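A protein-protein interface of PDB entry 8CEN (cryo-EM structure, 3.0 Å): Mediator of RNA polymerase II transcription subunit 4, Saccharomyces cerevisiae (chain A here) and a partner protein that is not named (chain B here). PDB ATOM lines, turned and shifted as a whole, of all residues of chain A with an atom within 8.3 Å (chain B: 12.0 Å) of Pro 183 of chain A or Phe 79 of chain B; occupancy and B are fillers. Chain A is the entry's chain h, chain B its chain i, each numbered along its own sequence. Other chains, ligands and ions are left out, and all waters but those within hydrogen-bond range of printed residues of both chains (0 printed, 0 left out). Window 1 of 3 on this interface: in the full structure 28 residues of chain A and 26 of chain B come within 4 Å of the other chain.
The backbone carbonyl oxygen of Phe 79 of chain B is in hydrogen-bond range of the guanidinium group of Arg 190 of chain A (3.1 Å).
OE2 of Glu 185 of chain A lies close to O of Leu 12 of chain B (2.8 Å).
The side-chain sulfur (SD) of Met 192 of chain A sits close to the backbone carbonyl oxygen (O) of Arg 77 of chain B.
OG of Ser 81 of chain B is in hydrogen-bond range of NE1 of Trp 83 of chain B, at 2.8 Å.
OD2 of Asp 186 of chain A lies within salt-bridge range of NH1 of Arg 190 of chain A, at 2.9 Å.
The side-chain carboxylate (OE2) of Glu 185 of chain A lies within salt-bridge range of the guanidinium group (NH1) of Arg 189 of chain A, 2.5 Å away.
The backbone NH (N) of Trp 83 of chain B sits at hydrogen-bond distance from the backbone carbonyl oxygen (O) of Tyr 76 of chain B.
O of Ala 78 of chain B lies within hydrogen-bond range of NE1 of Trp 83 of chain B, at 2.8 Å.
Among the printed residues, pairs that only touch across the chains: Arg 189 of chain A with Leu 12 of chain B, Leu 188 of chain A with Pro 14 of chain B, Phe 163 of chain A with Trp 83 of chain B, Pro 183 of chain A with Phe 79 of chain B, Glu 185 of chain A with Tyr 13 of chain B, Gly 191 of chain A with Phe 79 of chain B, Leu 193 of chain A with Pro 17 of chain B, Ala 187 of chain A with Phe 79 of chain B, Arg 190 of chain A with Gly 80 of chain B, Gly 191 of chain A with Gly 80 of chain B, Leu 193 of chain A with Pro 15 of chain B and Leu 188 of chain A with Tyr 13 of chain B.
Pro 183 of chain A touches just one residue of chain B: Phe 79 (3.6 Å).
Phe 79 of chain B touches just these residues of chain A: Pro 183, Ala 187, Arg 190 and Gly 191.
No residue of chain B comes within 4 Å of Ala 184 of chain A.
No residue of chain B comes within 4 Å of Asp 186 of chain A.
Of chain B, only Tyr 13 and Pro 14 come within 4 Å of Leu 188 of chain A.
Arg 190 of chain A touches two residues of chain B.
Gly 80 of chain B touches two residues of chain A.
Printed residues of chain B within 4 Å of Leu 193 of chain A: Pro 15 (3.9 Å) and Pro 17 (3.7 Å).
Printed residues of chain B within 4 Å of Glu 185 of chain A: Leu 12 (2.8 Å) and Tyr 13 (3.6 Å).
Of the printed residues of chain A, Pro 15 of chain B touches Leu 193 (3.9 Å).
The nearest residue of chain B that does not touch Pro 183 of chain A is Tyr 13 of chain B (6.4 Å).
The nearest residue of chain A that does not touch Phe 79 of chain B is Leu 188 of chain A (4.1 Å).
Printed residues of chain B that touch a printed residue of chain A: Leu 12, Tyr 13, Pro 14, Pro 15, Pro 17, Arg 77, Phe 79, Gly 80 and Trp 83.
Hydrophobic or aromatic side chains of chain A within 4 Å of the printed part of chain B: Phe 163, Pro 183, Leu 188, Met 192 and Leu 193.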
ATOM      1  N   PHE A 163     -13.755 -35.985  15.712  1.00  0.00           N
ATOM      2  CA  PHE A 163     -14.980 -35.743  14.961  1.00  0.00           C
ATOM      3  C   PHE A 163     -16.148 -36.604  15.414  1.00  0.00           C
ATOM      4  O   PHE A 163     -17.233 -36.076  15.680  1.00  0.00           O
ATOM      5  CB  PHE A 163     -14.716 -35.959  13.465  1.00  0.00           C
ATOM      6  CG  PHE A 163     -13.878 -34.883  12.844  1.00  0.00           C
ATOM      7  CD1 PHE A 163     -14.459 -33.710  12.395  1.00  0.00           C
ATOM      8  CD2 PHE A 163     -12.506 -35.033  12.733  1.00  0.00           C
ATOM      9  CE1 PHE A 163     -13.693 -32.714  11.829  1.00  0.00           C
ATOM     10  CE2 PHE A 163     -11.731 -34.037  12.169  1.00  0.00           C
ATOM     11  CZ  PHE A 163     -12.326 -32.877  11.717  1.00  0.00           C
ATOM     12  N   PRO A 177     -23.760 -30.532  16.896  1.00  0.00           N
ATOM     13  CA  PRO A 177     -23.401 -31.624  15.984  1.00  0.00           C
ATOM     14  C   PRO A 177     -23.100 -31.147  14.572  1.00  0.00           C
ATOM     15  O   PRO A 177     -23.091 -31.944  13.629  1.00  0.00           O
ATOM     16  CB  PRO A 177     -24.653 -32.504  16.016  1.00  0.00           C
ATOM     17  CG  PRO A 177     -25.748 -31.548  16.227  1.00  0.00           C
ATOM     18  CD  PRO A 177     -25.216 -30.442  17.093  1.00  0.00           C
ATOM     19  N   ASN A 178     -22.847 -29.845  14.426  1.00  0.00           N
ATOM     20  CA  ASN A 178     -22.914 -29.201  13.118  1.00  0.00           C
ATOM     21  C   ASN A 178     -21.747 -29.584  12.221  1.00  0.00           C
ATOM     22  O   ASN A 178     -21.935 -29.797  11.020  1.00  0.00           O
ATOM     23  CB  ASN A 178     -22.973 -27.690  13.297  1.00  0.00           C
ATOM     24  CG  ASN A 178     -24.297 -27.237  13.841  1.00  0.00           C
ATOM     25  OD1 ASN A 178     -24.436 -27.009  15.041  1.00  0.00           O
ATOM     26  ND2 ASN A 178     -25.288 -27.119  12.965  1.00  0.00           N
ATOM     27  N   ASN A 179     -20.534 -29.651  12.768  1.00  0.00           N
ATOM     28  CA  ASN A 179     -19.359 -29.985  11.970  1.00  0.00           C
ATOM     29  C   ASN A 179     -18.619 -31.200  12.513  1.00  0.00           C
ATOM     30  O   ASN A 179     -17.425 -31.368  12.246  1.00  0.00           O
ATOM     31  CB  ASN A 179     -18.419 -28.786  11.868  1.00  0.00           C
ATOM     32  CG  ASN A 179     -18.964 -27.695  10.971  1.00  0.00           C
ATOM     33  OD1 ASN A 179     -18.813 -27.749   9.753  1.00  0.00           O
ATOM     34  ND2 ASN A 179     -19.601 -26.696  11.570  1.00  0.00           N
ATOM     35  N   PHE A 180     -19.306 -32.055  13.267  1.00  0.00           N
ATOM     36  CA  PHE A 180     -18.723 -33.270  13.816  1.00  0.00           C
ATOM     37  C   PHE A 180     -19.213 -34.520  13.098  1.00  0.00           C
ATOM     38  O   PHE A 180     -18.406 -35.359  12.690  1.00  0.00           O
ATOM     39  CB  PHE A 180     -19.035 -33.372  15.313  1.00  0.00           C
ATOM     40  CG  PHE A 180     -18.331 -32.345  16.153  1.00  0.00           C
ATOM     41  CD1 PHE A 180     -18.850 -31.070  16.295  1.00  0.00           C
ATOM     42  CD2 PHE A 180     -17.150 -32.658  16.802  1.00  0.00           C
ATOM     43  CE1 PHE A 180     -18.206 -30.127  17.067  1.00  0.00           C
ATOM     44  CE2 PHE A 180     -16.501 -31.717  17.575  1.00  0.00           C
ATOM     45  CZ  PHE A 180     -17.031 -30.451  17.710  1.00  0.00           C
ATOM     46  N   ILE A 181     -20.525 -34.657  12.931  1.00  0.00           N
ATOM     47  CA  ILE A 181     -21.085 -35.804  12.228  1.00  0.00           C
ATOM     48  C   ILE A 181     -21.088 -35.554  10.731  1.00  0.00           C
ATOM     49  O   ILE A 181     -20.776 -36.446   9.940  1.00  0.00           O
ATOM     50  CB  ILE A 181     -22.516 -36.134  12.716  1.00  0.00           C
ATOM     51  CG1 ILE A 181     -22.575 -36.526  14.186  1.00  0.00           C
ATOM     52  CG2 ILE A 181     -23.091 -37.276  11.938  1.00  0.00           C
ATOM     53  CD1 ILE A 181     -22.770 -35.375  15.085  1.00  0.00           C
ATOM     54  N   TRP A 182     -21.439 -34.341  10.340  1.00  0.00           N
ATOM     55  CA  TRP A 182     -21.641 -33.960   8.955  1.00  0.00           C
ATOM     56  C   TRP A 182     -20.973 -32.617   8.720  1.00  0.00           C
ATOM     57  O   TRP A 182     -20.703 -31.882   9.674  1.00  0.00           O
ATOM     58  CB  TRP A 182     -23.138 -33.886   8.622  1.00  0.00           C
ATOM     59  CG  TRP A 182     -23.968 -33.038   9.545  1.00  0.00           C
ATOM     60  CD1 TRP A 182     -23.988 -31.677   9.616  1.00  0.00           C
ATOM     61  CD2 TRP A 182     -24.930 -33.499  10.502  1.00  0.00           C
ATOM     62  NE1 TRP A 182     -24.882 -31.263  10.570  1.00  0.00           N
ATOM     63  CE2 TRP A 182     -25.476 -32.364  11.127  1.00  0.00           C
ATOM     64  CE3 TRP A 182     -25.377 -34.764  10.893  1.00  0.00           C
ATOM     65  CZ2 TRP A 182     -26.444 -32.454  12.125  1.00  0.00           C
ATOM     66  CZ3 TRP A 182     -26.336 -34.852  11.885  1.00  0.00           C
ATOM     67  CH2 TRP A 182     -26.859 -33.705  12.489  1.00  0.00           C
ATOM     68  N   PRO A 183     -20.657 -32.284   7.469  1.00  0.00           N
ATOM     69  CA  PRO A 183     -20.256 -30.906   7.163  1.00  0.00           C
ATOM     70  C   PRO A 183     -21.469 -29.987   7.196  1.00  0.00           C
ATOM     71  O   PRO A 183     -22.501 -30.274   6.586  1.00  0.00           O
ATOM     72  CB  PRO A 183     -19.665 -31.008   5.753  1.00  0.00           C
ATOM     73  CG  PRO A 183     -20.262 -32.233   5.178  1.00  0.00           C
ATOM     74  CD  PRO A 183     -20.473 -33.180   6.317  1.00  0.00           C
ATOM     75  N   ALA A 184     -21.341 -28.880   7.921  1.00  0.00           N
ATOM     76  CA  ALA A 184     -22.445 -27.948   8.073  1.00  0.00           C
ATOM     77  C   ALA A 184     -22.630 -27.130   6.798  1.00  0.00           C
ATOM     78  O   ALA A 184     -21.888 -27.269   5.819  1.00  0.00           O
ATOM     79  CB  ALA A 184     -22.213 -27.038   9.276  1.00  0.00           C
ATOM     80  N   GLU A 185     -23.648 -26.263   6.820  1.00  0.00           N
ATOM     81  CA  GLU A 185     -23.913 -25.394   5.679  1.00  0.00           C
ATOM     82  C   GLU A 185     -22.735 -24.473   5.411  1.00  0.00           C
ATOM     83  O   GLU A 185     -22.293 -24.341   4.266  1.00  0.00           O
ATOM     84  CB  GLU A 185     -25.184 -24.575   5.915  1.00  0.00           C
ATOM     85  CG  GLU A 185     -25.833 -24.044   4.636  1.00  0.00           C
ATOM     86  CD  GLU A 185     -25.289 -22.688   4.191  1.00  0.00           C
ATOM     87  OE1 GLU A 185     -24.409 -22.126   4.863  1.00  0.00           O
ATOM     88  OE2 GLU A 185     -25.733 -22.176   3.147  1.00  0.00           O
ATOM     89  N   ASP A 186     -22.225 -23.813   6.457  1.00  0.00           N
ATOM     90  CA  ASP A 186     -21.090 -22.913   6.288  1.00  0.00           C
ATOM     91  C   ASP A 186     -19.853 -23.663   5.822  1.00  0.00           C
ATOM     92  O   ASP A 186     -19.046 -23.114   5.065  1.00  0.00           O
ATOM     93  CB  ASP A 186     -20.800 -22.171   7.591  1.00  0.00           C
ATOM     94  CG  ASP A 186     -20.760 -23.096   8.790  1.00  0.00           C
ATOM     95  OD1 ASP A 186     -21.776 -23.774   9.048  1.00  0.00           O
ATOM     96  OD2 ASP A 186     -19.714 -23.149   9.471  1.00  0.00           O
ATOM     97  N   ALA A 187     -19.701 -24.920   6.252  1.00  0.00           N
ATOM     98  CA  ALA A 187     -18.619 -25.759   5.752  1.00  0.00           C
ATOM     99  C   ALA A 187     -18.761 -26.011   4.259  1.00  0.00           C
ATOM    100  O   ALA A 187     -17.772 -25.966   3.522  1.00  0.00           O
ATOM    101  CB  ALA A 187     -18.583 -27.081   6.515  1.00  0.00           C
ATOM    102  N   LEU A 188     -19.985 -26.269   3.788  1.00  0.00           N
ATOM    103  CA  LEU A 188     -20.179 -26.479   2.355  1.00  0.00           C
ATOM    104  C   LEU A 188     -20.017 -25.187   1.560  1.00  0.00           C
ATOM    105  O   LEU A 188     -19.615 -25.228   0.392  1.00  0.00           O
ATOM    106  CB  LEU A 188     -21.548 -27.104   2.091  1.00  0.00           C
ATOM    107  CG  LEU A 188     -21.789 -28.456   2.762  1.00  0.00           C
ATOM    108  CD1 LEU A 188     -23.223 -28.923   2.572  1.00  0.00           C
ATOM    109  CD2 LEU A 188     -20.808 -29.489   2.238  1.00  0.00           C
ATOM    110  N   ARG A 189     -20.325 -24.040   2.168  1.00  0.00           N
ATOM    111  CA  ARG A 189     -20.147 -22.760   1.483  1.00  0.00           C
ATOM    112  C   ARG A 189     -18.672 -22.404   1.350  1.00  0.00           C
ATOM    113  O   ARG A 189     -18.174 -22.177   0.241  1.00  0.00           O
ATOM    114  CB  ARG A 189     -20.883 -21.646   2.223  1.00  0.00           C
ATOM    115  CG  ARG A 189     -22.366 -21.841   2.384  1.00  0.00           C
ATOM    116  CD  ARG A 189     -23.163 -21.511   1.135  1.00  0.00           C
ATOM    117  NE  ARG A 189     -23.397 -20.079   0.978  1.00  0.00           N
ATOM    118  CZ  ARG A 189     -24.166 -19.327   1.758  1.00  0.00           C
ATOM    119  NH1 ARG A 189     -24.828 -19.834   2.785  1.00  0.00           N
ATOM    120  NH2 ARG A 189     -24.273 -18.027   1.498  1.00  0.00           N
ATOM    121  N   ARG A 190     -17.953 -22.333   2.476  1.00  0.00           N
ATOM    122  CA  ARG A 190     -16.533 -22.004   2.425  1.00  0.00           C
ATOM    123  C   ARG A 190     -15.703 -23.133   1.838  1.00  0.00           C
ATOM    124  O   ARG A 190     -14.534 -22.913   1.504  1.00  0.00           O
ATOM    125  CB  ARG A 190     -15.989 -21.662   3.812  1.00  0.00           C
ATOM    126  CG  ARG A 190     -15.886 -22.849   4.750  1.00  0.00           C
ATOM    127  CD  ARG A 190     -15.351 -22.446   6.110  1.00  0.00           C
ATOM    128  NE  ARG A 190     -15.215 -23.594   6.995  1.00  0.00           N
ATOM    129  CZ  ARG A 190     -16.160 -24.017   7.824  1.00  0.00           C
ATOM    130  NH1 ARG A 190     -17.322 -23.393   7.923  1.00  0.00           N
ATOM    131  NH2 ARG A 190     -15.932 -25.091   8.575  1.00  0.00           N
ATOM    132  N   GLY A 191     -16.276 -24.323   1.704  1.00  0.00           N
ATOM    133  CA  GLY A 191     -15.604 -25.406   1.033  1.00  0.00           C
ATOM    134  C   GLY A 191     -15.503 -25.156  -0.451  1.00  0.00           C
ATOM    135  O   GLY A 191     -16.065 -24.213  -1.011  1.00  0.00           O
ATOM    136  N   MET A 192     -14.771 -26.041  -1.107  1.00  0.00           N
ATOM    137  CA  MET A 192     -14.320 -25.793  -2.460  1.00  0.00           C
ATOM    138  C   MET A 192     -15.078 -26.601  -3.503  1.00  0.00           C
ATOM    139  O   MET A 192     -14.807 -26.455  -4.699  1.00  0.00           O
ATOM    140  CB  MET A 192     -12.816 -26.045  -2.517  1.00  0.00           C
ATOM    141  CG  MET A 192     -12.414 -27.464  -2.262  1.00  0.00           C
ATOM    142  SD  MET A 192     -10.635 -27.542  -2.363  1.00  0.00           S
ATOM    143  CE  MET A 192     -10.404 -27.340  -4.103  1.00  0.00           C
ATOM    144  N   LEU A 193     -16.047 -27.419  -3.085  1.00  0.00           N
ATOM    145  CA  LEU A 193     -17.097 -27.852  -4.001  1.00  0.00           C
ATOM    146  C   LEU A 193     -17.944 -26.662  -4.440  1.00  0.00           C
ATOM    147  O   LEU A 193     -18.403 -26.597  -5.590  1.00  0.00           O
ATOM    148  CB  LEU A 193     -17.960 -28.922  -3.331  1.00  0.00           C
ATOM    149  CG  LEU A 193     -19.277 -29.349  -3.988  1.00  0.00           C
ATOM    150  CD1 LEU A 193     -19.039 -29.905  -5.378  1.00  0.00           C
ATOM    151  CD2 LEU A 193     -20.007 -30.363  -3.121  1.00  0.00           C
ATOM    152  N   LEU B  12     -29.086 -22.087  -1.063  1.00  0.00           N
ATOM    153  CA  LEU B  12     -28.359 -22.326   0.180  1.00  0.00           C
ATOM    154  C   LEU B  12     -27.195 -23.283  -0.030  1.00  0.00           C
ATOM    155  O   LEU B  12     -26.091 -23.048   0.474  1.00  0.00           O
ATOM    156  CB  LEU B  12     -29.307 -22.875   1.241  1.00  0.00           C
ATOM    157  CG  LEU B  12     -28.826 -22.903   2.692  1.00  0.00           C
ATOM    158  CD1 LEU B  12     -29.007 -21.549   3.353  1.00  0.00           C
ATOM    159  CD2 LEU B  12     -29.513 -23.998   3.495  1.00  0.00           C
ATOM    160  N   TYR B  13     -27.413 -24.351  -0.778  1.00  0.00           N
ATOM    161  CA  TYR B  13     -26.434 -25.416  -0.863  1.00  0.00           C
ATOM    162  C   TYR B  13     -25.748 -25.426  -2.225  1.00  0.00           C
ATOM    163  O   TYR B  13     -26.351 -25.040  -3.232  1.00  0.00           O
ATOM    164  CB  TYR B  13     -27.103 -26.774  -0.623  1.00  0.00           C
ATOM    165  CG  TYR B  13     -27.505 -27.013   0.813  1.00  0.00           C
ATOM    166  CD1 TYR B  13     -26.566 -26.969   1.833  1.00  0.00           C
ATOM    167  CD2 TYR B  13     -28.825 -27.282   1.149  1.00  0.00           C
ATOM    168  CE1 TYR B  13     -26.929 -27.189   3.148  1.00  0.00           C
ATOM    169  CE2 TYR B  13     -29.198 -27.504   2.460  1.00  0.00           C
ATOM    170  CZ  TYR B  13     -28.245 -27.455   3.454  1.00  0.00           C
ATOM    171  OH  TYR B  13     -28.609 -27.674   4.763  1.00  0.00           O
ATOM    172  N   PRO B  14     -24.481 -25.843  -2.286  1.00  0.00           N
ATOM    173  CA  PRO B  14     -23.824 -25.980  -3.583  1.00  0.00           C
ATOM    174  C   PRO B  14     -24.427 -27.123  -4.377  1.00  0.00           C
ATOM    175  O   PRO B  14     -24.946 -28.093  -3.800  1.00  0.00           O
ATOM    176  CB  PRO B  14     -22.358 -26.271  -3.208  1.00  0.00           C
ATOM    177  CG  PRO B  14     -22.216 -25.799  -1.802  1.00  0.00           C
ATOM    178  CD  PRO B  14     -23.545 -26.045  -1.168  1.00  0.00           C
ATOM    179  N   PRO B  15     -24.389 -27.053  -5.704  1.00  0.00           N
ATOM    180  CA  PRO B  15     -24.904 -28.152  -6.525  1.00  0.00           C
ATOM    181  C   PRO B  15     -23.947 -29.330  -6.523  1.00  0.00           C
ATOM    182  O   PRO B  15     -22.820 -29.221  -6.016  1.00  0.00           O
ATOM    183  CB  PRO B  15     -25.014 -27.519  -7.922  1.00  0.00           C
ATOM    184  CG  PRO B  15     -24.016 -26.431  -7.915  1.00  0.00           C
ATOM    185  CD  PRO B  15     -24.008 -25.887  -6.518  1.00  0.00           C
ATOM    186  N   PRO B  17     -21.204 -31.937  -8.258  1.00  0.00           N
ATOM    187  CA  PRO B  17     -20.088 -31.549  -9.121  1.00  0.00           C
ATOM    188  C   PRO B  17     -20.441 -31.696 -10.590  1.00  0.00           C
ATOM    189  O   PRO B  17     -21.203 -32.602 -10.975  1.00  0.00           O
ATOM    190  CB  PRO B  17     -18.970 -32.528  -8.716  1.00  0.00           C
ATOM    191  CG  PRO B  17     -19.343 -33.006  -7.370  1.00  0.00           C
ATOM    192  CD  PRO B  17     -20.833 -33.046  -7.360  1.00  0.00           C
ATOM    193  N   GLN B  75      -1.318 -33.463   0.703  1.00  0.00           N
ATOM    194  CA  GLN B  75      -2.201 -32.513   1.360  1.00  0.00           C
ATOM    195  C   GLN B  75      -3.363 -32.208   0.430  1.00  0.00           C
ATOM    196  O   GLN B  75      -3.170 -31.993  -0.771  1.00  0.00           O
ATOM    197  CB  GLN B  75      -1.477 -31.213   1.719  1.00  0.00           C
ATOM    198  CG  GLN B  75      -0.179 -31.398   2.475  1.00  0.00           C
ATOM    199  CD  GLN B  75       0.571 -30.095   2.654  1.00  0.00           C
ATOM    200  OE1 GLN B  75       1.554 -29.831   1.964  1.00  0.00           O
ATOM    201  NE2 GLN B  75       0.104 -29.268   3.581  1.00  0.00           N
ATOM    202  N   TYR B  76      -4.567 -32.192   0.986  1.00  0.00           N
ATOM    203  CA  TYR B  76      -5.760 -31.868   0.222  1.00  0.00           C
ATOM    204  C   TYR B  76      -6.602 -30.853   0.981  1.00  0.00           C
ATOM    205  O   TYR B  76      -6.580 -30.795   2.212  1.00  0.00           O
ATOM    206  CB  TYR B  76      -6.590 -33.126  -0.102  1.00  0.00           C
ATOM    207  CG  TYR B  76      -7.158 -33.862   1.092  1.00  0.00           C
ATOM    208  CD1 TYR B  76      -6.376 -34.745   1.826  1.00  0.00           C
ATOM    209  CD2 TYR B  76      -8.481 -33.687   1.474  1.00  0.00           C
ATOM    210  CE1 TYR B  76      -6.893 -35.423   2.912  1.00  0.00           C
ATOM    211  CE2 TYR B  76      -9.006 -34.360   2.559  1.00  0.00           C
ATOM    212  CZ  TYR B  76      -8.209 -35.229   3.272  1.00  0.00           C
ATOM    213  OH  TYR B  76      -8.729 -35.901   4.354  1.00  0.00           O
ATOM    214  N   ARG B  77      -7.343 -30.048   0.234  1.00  0.00           N
ATOM    215  CA  ARG B  77      -8.168 -29.000   0.809  1.00  0.00           C
ATOM    216  C   ARG B  77      -9.624 -29.442   0.830  1.00  0.00           C
ATOM    217  O   ARG B  77     -10.138 -29.967  -0.162  1.00  0.00           O
ATOM    218  CB  ARG B  77      -8.027 -27.703   0.015  1.00  0.00           C
ATOM    219  CG  ARG B  77      -6.729 -26.961   0.236  1.00  0.00           C
ATOM    220  CD  ARG B  77      -6.661 -25.736  -0.654  1.00  0.00           C
ATOM    221  NE  ARG B  77      -7.129 -26.031  -2.003  1.00  0.00           N
ATOM    222  CZ  ARG B  77      -6.390 -25.913  -3.097  1.00  0.00           C
ATOM    223  NH1 ARG B  77      -5.132 -25.509  -3.042  1.00  0.00           N
ATOM    224  NH2 ARG B  77      -6.927 -26.209  -4.277  1.00  0.00           N
ATOM    225  N   ALA B  78     -10.283 -29.230   1.968  1.00  0.00           N
ATOM    226  CA  ALA B  78     -11.690 -29.579   2.114  1.00  0.00           C
ATOM    227  C   ALA B  78     -12.298 -28.717   3.209  1.00  0.00           C
ATOM    228  O   ALA B  78     -11.707 -28.580   4.285  1.00  0.00           O
ATOM    229  CB  ALA B  78     -11.865 -31.064   2.446  1.00  0.00           C
ATOM    230  N   PHE B  79     -13.471 -28.143   2.920  1.00  0.00           N
ATOM    231  CA  PHE B  79     -14.260 -27.346   3.867  1.00  0.00           C
ATOM    232  C   PHE B  79     -13.471 -26.155   4.409  1.00  0.00           C
ATOM    233  O   PHE B  79     -13.590 -25.789   5.579  1.00  0.00           O
ATOM    234  CB  PHE B  79     -14.795 -28.214   5.007  1.00  0.00           C
ATOM    235  CG  PHE B  79     -15.374 -29.518   4.544  1.00  0.00           C
ATOM    236  CD1 PHE B  79     -16.518 -29.548   3.764  1.00  0.00           C
ATOM    237  CD2 PHE B  79     -14.765 -30.716   4.878  1.00  0.00           C
ATOM    238  CE1 PHE B  79     -17.046 -30.750   3.331  1.00  0.00           C
ATOM    239  CE2 PHE B  79     -15.289 -31.920   4.450  1.00  0.00           C
ATOM    240  CZ  PHE B  79     -16.431 -31.937   3.676  1.00  0.00           C
ATOM    241  N   GLY B  80     -12.675 -25.536   3.543  1.00  0.00           N
ATOM    242  CA  GLY B  80     -11.874 -24.389   3.933  1.00  0.00           C
ATOM    243  C   GLY B  80     -10.774 -24.697   4.924  1.00  0.00           C
ATOM    244  O   GLY B  80     -10.531 -23.904   5.843  1.00  0.00           O
ATOM    245  N   SER B  81     -10.100 -25.832   4.762  1.00  0.00           N
ATOM    246  CA  SER B  81      -9.035 -26.227   5.671  1.00  0.00           C
ATOM    247  C   SER B  81      -8.060 -27.130   4.930  1.00  0.00           C
ATOM    248  O   SER B  81      -8.366 -27.663   3.862  1.00  0.00           O
ATOM    249  CB  SER B  81      -9.588 -26.936   6.911  1.00  0.00           C
ATOM    250  OG  SER B  81     -10.239 -28.142   6.557  1.00  0.00           O
ATOM    251  N   ILE B  82      -6.876 -27.290   5.513  1.00  0.00           N
ATOM    252  CA  ILE B  82      -5.822 -28.128   4.953  1.00  0.00           C
ATOM    253  C   ILE B  82      -5.815 -29.450   5.703  1.00  0.00           C
ATOM    254  O   ILE B  82      -5.851 -29.467   6.940  1.00  0.00           O
ATOM    255  CB  ILE B  82      -4.450 -27.441   5.050  1.00  0.00           C
ATOM    256  CG1 ILE B  82      -4.544 -25.974   4.626  1.00  0.00           C
ATOM    257  CG2 ILE B  82      -3.429 -28.176   4.195  1.00  0.00           C
ATOM    258  CD1 ILE B  82      -4.870 -25.772   3.172  1.00  0.00           C
ATOM    259  N   TRP B  83      -5.763 -30.556   4.967  1.00  0.00           N
ATOM    260  CA  TRP B  83      -5.706 -31.883   5.553  1.00  0.00           C
ATOM    261  C   TRP B  83      -4.528 -32.624   4.946  1.00  0.00           C
ATOM    262  O   TRP B  83      -4.078 -32.313   3.841  1.00  0.00           O
ATOM    263  CB  TRP B  83      -6.986 -32.690   5.295  1.00  0.00           C
ATOM    264  CG  TRP B  83      -8.281 -31.981   5.550  1.00  0.00           C
ATOM    265  CD1 TRP B  83      -8.858 -31.019   4.774  1.00  0.00           C
ATOM    266  CD2 TRP B  83      -9.185 -32.213   6.637  1.00  0.00           C
ATOM    267  NE1 TRP B  83     -10.052 -30.623   5.320  1.00  0.00           N
ATOM    268  CE2 TRP B  83     -10.278 -31.341   6.464  1.00  0.00           C
ATOM    269  CE3 TRP B  83      -9.171 -33.065   7.744  1.00  0.00           C
ATOM    270  CZ2 TRP B  83     -11.347 -31.300   7.354  1.00  0.00           C
ATOM    271  CZ3 TRP B  83     -10.228 -33.018   8.629  1.00  0.00           C
ATOM    272  CH2 TRP B  83     -11.304 -32.146   8.427  1.00  0.00           C
ATOM    273  N   GLN B  84      -4.051 -33.634   5.664  1.00  0.00           N
ATOM    274  CA  GLN B  84      -2.957 -34.470   5.199  1.00  0.00           C
ATOM    275  C   GLN B  84      -3.391 -35.928   5.197  1.00  0.00           C
ATOM    276  O   GLN B  84      -4.207 -36.350   6.022  1.00  0.00           O
ATOM    277  CB  GLN B  84      -1.715 -34.281   6.072  1.00  0.00           C
ATOM    278  CG  GLN B  84      -0.989 -32.974   5.805  1.00  0.00           C
ATOM    279  CD  GLN B  84      -0.557 -32.276   7.075  1.00  0.00           C
ATOM    280  OE1 GLN B  84      -0.718 -32.805   8.174  1.00  0.00           O
ATOM    281  NE2 GLN B  84      -0.011 -31.074   6.933  1.00  0.00           N
